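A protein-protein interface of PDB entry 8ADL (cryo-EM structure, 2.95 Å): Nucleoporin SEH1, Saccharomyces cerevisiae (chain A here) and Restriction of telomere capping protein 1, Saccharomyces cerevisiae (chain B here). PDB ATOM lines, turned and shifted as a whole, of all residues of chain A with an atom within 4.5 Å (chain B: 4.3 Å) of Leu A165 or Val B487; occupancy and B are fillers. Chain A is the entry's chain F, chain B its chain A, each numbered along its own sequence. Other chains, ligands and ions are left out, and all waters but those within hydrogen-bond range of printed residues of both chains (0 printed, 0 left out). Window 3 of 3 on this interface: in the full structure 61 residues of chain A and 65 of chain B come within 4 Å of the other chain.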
ATOM      1  N   ASN A 163       0.400  -2.982  31.100  1.00  0.00           N
ATOM      2  CA  ASN A 163      -0.383  -3.712  30.105  1.00  0.00           C
ATOM      3  C   ASN A 163      -1.752  -3.053  30.005  1.00  0.00           C
ATOM      4  O   ASN A 163      -2.696  -3.416  30.708  1.00  0.00           O
ATOM      5  CB  ASN A 163      -0.494  -5.185  30.477  1.00  0.00           C
ATOM      6  CG  ASN A 163      -0.884  -6.055  29.297  1.00  0.00           C
ATOM      7  OD1 ASN A 163      -0.958  -5.584  28.163  1.00  0.00           O
ATOM      8  ND2 ASN A 163      -1.133  -7.332  29.561  1.00  0.00           N
ATOM      9  N   HIS A 164      -1.858  -2.061  29.120  1.00  0.00           N
ATOM     10  CA  HIS A 164      -3.086  -1.282  29.021  1.00  0.00           C
ATOM     11  C   HIS A 164      -4.195  -2.050  28.315  1.00  0.00           C
ATOM     12  O   HIS A 164      -5.375  -1.839  28.617  1.00  0.00           O
ATOM     13  CB  HIS A 164      -2.817   0.036  28.294  1.00  0.00           C
ATOM     14  CG  HIS A 164      -2.083   1.043  29.124  1.00  0.00           C
ATOM     15  ND1 HIS A 164      -2.729   1.972  29.910  1.00  0.00           N
ATOM     16  CD2 HIS A 164      -0.757   1.266  29.289  1.00  0.00           C
ATOM     17  CE1 HIS A 164      -1.834   2.724  30.524  1.00  0.00           C
ATOM     18  NE2 HIS A 164      -0.630   2.317  30.164  1.00  0.00           N
ATOM     19  N   LEU A 165      -3.843  -2.933  27.376  1.00  0.00           N
ATOM     20  CA  LEU A 165      -4.863  -3.617  26.590  1.00  0.00           C
ATOM     21  C   LEU A 165      -5.572  -4.694  27.400  1.00  0.00           C
ATOM     22  O   LEU A 165      -6.727  -5.026  27.108  1.00  0.00           O
ATOM     23  CB  LEU A 165      -4.239  -4.222  25.333  1.00  0.00           C
ATOM     24  CG  LEU A 165      -5.187  -4.570  24.184  1.00  0.00           C
ATOM     25  CD1 LEU A 165      -6.180  -3.447  23.938  1.00  0.00           C
ATOM     26  CD2 LEU A 165      -4.396  -4.879  22.922  1.00  0.00           C
ATOM     27  N   GLN A 166      -4.909  -5.248  28.413  1.00  0.00           N
ATOM     28  CA  GLN A 166      -5.523  -6.242  29.292  1.00  0.00           C
ATOM     29  C   GLN A 166      -5.899  -5.552  30.599  1.00  0.00           C
ATOM     30  O   GLN A 166      -5.186  -5.614  31.601  1.00  0.00           O
ATOM     31  CB  GLN A 166      -4.582  -7.421  29.513  1.00  0.00           C
ATOM     32  CG  GLN A 166      -4.576  -8.425  28.372  1.00  0.00           C
ATOM     33  CD  GLN A 166      -5.933  -9.067  28.155  1.00  0.00           C
ATOM     34  OE1 GLN A 166      -6.425  -9.139  27.030  1.00  0.00           O
ATOM     35  NE2 GLN A 166      -6.543  -9.542  29.235  1.00  0.00           N
ATOM     36  N   SER A 167      -7.052  -4.888  30.579  1.00  0.00           N
ATOM     37  CA  SER A 167      -7.599  -4.247  31.766  1.00  0.00           C
ATOM     38  C   SER A 167      -9.101  -4.099  31.586  1.00  0.00           C
ATOM     39  O   SER A 167      -9.616  -4.129  30.465  1.00  0.00           O
ATOM     40  CB  SER A 167      -6.948  -2.884  32.025  1.00  0.00           C
ATOM     41  OG  SER A 167      -7.246  -1.969  30.984  1.00  0.00           O
ATOM     42  N   GLU B 472      -0.779   6.116  19.279  1.00  0.00           N
ATOM     43  CA  GLU B 472      -0.611   4.714  19.631  1.00  0.00           C
ATOM     44  C   GLU B 472      -0.605   3.882  18.359  1.00  0.00           C
ATOM     45  O   GLU B 472      -1.148   4.286  17.327  1.00  0.00           O
ATOM     46  CB  GLU B 472      -1.719   4.238  20.580  1.00  0.00           C
ATOM     47  CG  GLU B 472      -3.124   4.445  20.035  1.00  0.00           C
ATOM     48  CD  GLU B 472      -4.200   4.099  21.043  1.00  0.00           C
ATOM     49  OE1 GLU B 472      -3.852   3.685  22.168  1.00  0.00           O
ATOM     50  OE2 GLU B 472      -5.396   4.241  20.710  1.00  0.00           O
ATOM     51  N   VAL B 473       0.017   2.709  18.442  1.00  0.00           N
ATOM     52  CA  VAL B 473       0.045   1.778  17.320  1.00  0.00           C
ATOM     53  C   VAL B 473      -1.267   1.001  17.321  1.00  0.00           C
ATOM     54  O   VAL B 473      -1.519   0.187  18.212  1.00  0.00           O
ATOM     55  CB  VAL B 473       1.249   0.834  17.401  1.00  0.00           C
ATOM     56  CG1 VAL B 473       1.236  -0.148  16.239  1.00  0.00           C
ATOM     57  CG2 VAL B 473       2.545   1.631  17.421  1.00  0.00           C
ATOM     58  N   PRO B 484     -10.396  -2.461  16.623  1.00  0.00           N
ATOM     59  CA  PRO B 484      -9.010  -2.783  16.277  1.00  0.00           C
ATOM     60  C   PRO B 484      -8.626  -4.167  16.779  1.00  0.00           C
ATOM     61  O   PRO B 484      -9.299  -4.768  17.619  1.00  0.00           O
ATOM     62  CB  PRO B 484      -8.200  -1.695  16.991  1.00  0.00           C
ATOM     63  CG  PRO B 484      -9.076  -1.239  18.103  1.00  0.00           C
ATOM     64  CD  PRO B 484     -10.486  -1.374  17.613  1.00  0.00           C
ATOM     65  N   HIS B 486      -5.065  -4.743  17.608  1.00  0.00           N
ATOM     66  CA  HIS B 486      -3.969  -4.513  18.539  1.00  0.00           C
ATOM     67  C   HIS B 486      -3.878  -3.023  18.819  1.00  0.00           C
ATOM     68  O   HIS B 486      -3.834  -2.216  17.887  1.00  0.00           O
ATOM     69  CB  HIS B 486      -2.636  -5.029  17.979  1.00  0.00           C
ATOM     70  CG  HIS B 486      -2.669  -6.468  17.564  1.00  0.00           C
ATOM     71  ND1 HIS B 486      -2.715  -7.505  18.469  1.00  0.00           N
ATOM     72  CD2 HIS B 486      -2.678  -7.040  16.336  1.00  0.00           C
ATOM     73  CE1 HIS B 486      -2.743  -8.655  17.820  1.00  0.00           C
ATOM     74  NE2 HIS B 486      -2.721  -8.401  16.524  1.00  0.00           N
ATOM     75  N   VAL B 487      -3.850  -2.666  20.103  1.00  0.00           N
ATOM     76  CA  VAL B 487      -3.819  -1.275  20.548  1.00  0.00           C
ATOM     77  C   VAL B 487      -2.485  -1.123  21.281  1.00  0.00           C
ATOM     78  O   VAL B 487      -2.425  -0.646  22.421  1.00  0.00           O
ATOM     79  CB  VAL B 487      -5.054  -0.915  21.408  1.00  0.00           C
ATOM     80  CG1 VAL B 487      -5.156   0.603  21.695  1.00  0.00           C
ATOM     81  CG2 VAL B 487      -6.328  -1.388  20.735  1.00  0.00           C
ATOM     82  N   LEU B 488      -1.436  -1.692  20.679  1.00  0.00           N
ATOM     83  CA  LEU B 488      -0.049  -1.564  21.120  1.00  0.00           C
ATOM     84  C   LEU B 488       0.300  -0.129  21.484  1.00  0.00           C
ATOM     85  O   LEU B 488       0.238   0.775  20.643  1.00  0.00           O
ATOM     86  CB  LEU B 488       0.884  -2.059  20.012  1.00  0.00           C
ATOM     87  CG  LEU B 488       0.582  -3.433  19.415  1.00  0.00           C
ATOM     88  CD1 LEU B 488       1.460  -3.694  18.201  1.00  0.00           C
ATOM     89  CD2 LEU B 488       0.774  -4.518  20.458  1.00  0.00           C
ATOM     90  N   LEU B 489       0.662   0.080  22.746  1.00  0.00           N
ATOM     91  CA  LEU B 489       0.775   1.409  23.325  1.00  0.00           C
ATOM     92  C   LEU B 489       2.089   1.521  24.083  1.00  0.00           C
ATOM     93  O   LEU B 489       2.521   0.569  24.740  1.00  0.00           O
ATOM     94  CB  LEU B 489      -0.431   1.691  24.248  1.00  0.00           C
ATOM     95  CG  LEU B 489      -0.690   3.052  24.902  1.00  0.00           C
ATOM     96  CD1 LEU B 489      -2.185   3.264  25.036  1.00  0.00           C
ATOM     97  CD2 LEU B 489      -0.059   3.125  26.281  1.00  0.00           C
ATOM     98  N   PRO B 523      -2.557 -10.264  22.939  1.00  0.00           N
ATOM     99  CA  PRO B 523      -3.991 -10.415  23.212  1.00  0.00           C
ATOM    100  C   PRO B 523      -4.834  -9.678  22.185  1.00  0.00           C
ATOM    101  O   PRO B 523      -4.438  -8.643  21.644  1.00  0.00           O
ATOM    102  CB  PRO B 523      -4.153  -9.806  24.612  1.00  0.00           C
ATOM    103  CG  PRO B 523      -2.918  -8.980  24.821  1.00  0.00           C
ATOM    104  CD  PRO B 523      -1.844  -9.729  24.109  1.00  0.00           C
ATOM    105  N   VAL B 525      -8.174  -7.548  21.085  1.00  0.00           N
ATOM    106  CA  VAL B 525      -9.041  -6.549  21.701  1.00  0.00           C
ATOM    107  C   VAL B 525     -10.485  -7.033  21.738  1.00  0.00           C
ATOM    108  O   VAL B 525     -11.251  -6.650  22.632  1.00  0.00           O
ATOM    109  CB  VAL B 525      -8.902  -5.215  20.942  1.00  0.00           C
ATOM    110  CG1 VAL B 525      -9.598  -4.074  21.678  1.00  0.00           C
ATOM    111  CG2 VAL B 525      -7.442  -4.899  20.716  1.00  0.00           C
ATOM    112  N   ASN B 528     -11.348  -9.106  24.999  1.00  0.00           N
ATOM    113  CA  ASN B 528     -11.433  -8.343  26.239  1.00  0.00           C
ATOM    114  C   ASN B 528     -12.701  -7.506  26.348  1.00  0.00           C
ATOM    115  O   ASN B 528     -13.066  -7.105  27.458  1.00  0.00           O
ATOM    116  CB  ASN B 528     -10.207  -7.437  26.375  1.00  0.00           C
ATOM    117  CG  ASN B 528      -9.991  -6.956  27.795  1.00  0.00           C
ATOM    118  OD1 ASN B 528      -9.579  -7.722  28.665  1.00  0.00           O
ATOM    119  ND2 ASN B 528     -10.271  -5.682  28.037  1.00  0.00           N
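Hydrophobic or aromatic side chains of chain A that line the printed part of chain B: His A164 and Leu A165. Printed residues of chain B that touch a printed residue of chain A: Val B487, Leu B489, Pro B523, Val B525 and Asn B528. Hydrophobic or aromatic side chains of chain B that line the printed part of chain A: Val B487, Leu B489, Pro B523 and Val B525. Among the printed residues, no Asp or Glu carboxylate lies within 4 Å of a Lys or Arg side-chain nitrogen of the other chain.
Printed residues of chain B within 4 Å of Leu A165: Val B487 (3.6 Å), Pro B523 (3.98 Å), Val B525 (3.8 Å) and Asn B528 (3.7 Å). Of the printed residues of chain B, Gln A166 touches Pro B523 and Asn B528. Printed residues of chain A within 4 Å of Leu B489: His A164. Of the printed residues of chain A, Pro B523 touches Leu A165 (3.98 Å) and Gln A166 (3.4 Å). Of the printed residues of chain A, Val B525 touches Leu A165 (3.8 Å). Of the printed residues of chain A, Asn B528 touches Leu A165 (3.7 Å), Gln A166 (3.6 Å) and Ser A167 (3.0 Å). The nearest printed residue of chain A that does not touch Val B487 is His A164 (5.9 Å). The nearest printed residue of chain B that does not touch Gln A166 is Val B525 (6.4 Å).
Among the printed residues, merely in contact across the chains: His A164 with Leu B489, Leu A165 with Val B487, Leu A165 with Pro B523, Leu A165 with Val B525, Leu A165 with Asn B528, Gln A166 with Pro B523 and Gln A166 with Asn B528.
The backbone carbonyl oxygen of Ser A167 sits at hydrogen-bond distance from the side-chain amide nitrogen of Asn B528 (3.0 Å).
O of His A164 sits at hydrogen-bond distance from OG of Ser A167 (3.0 Å).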
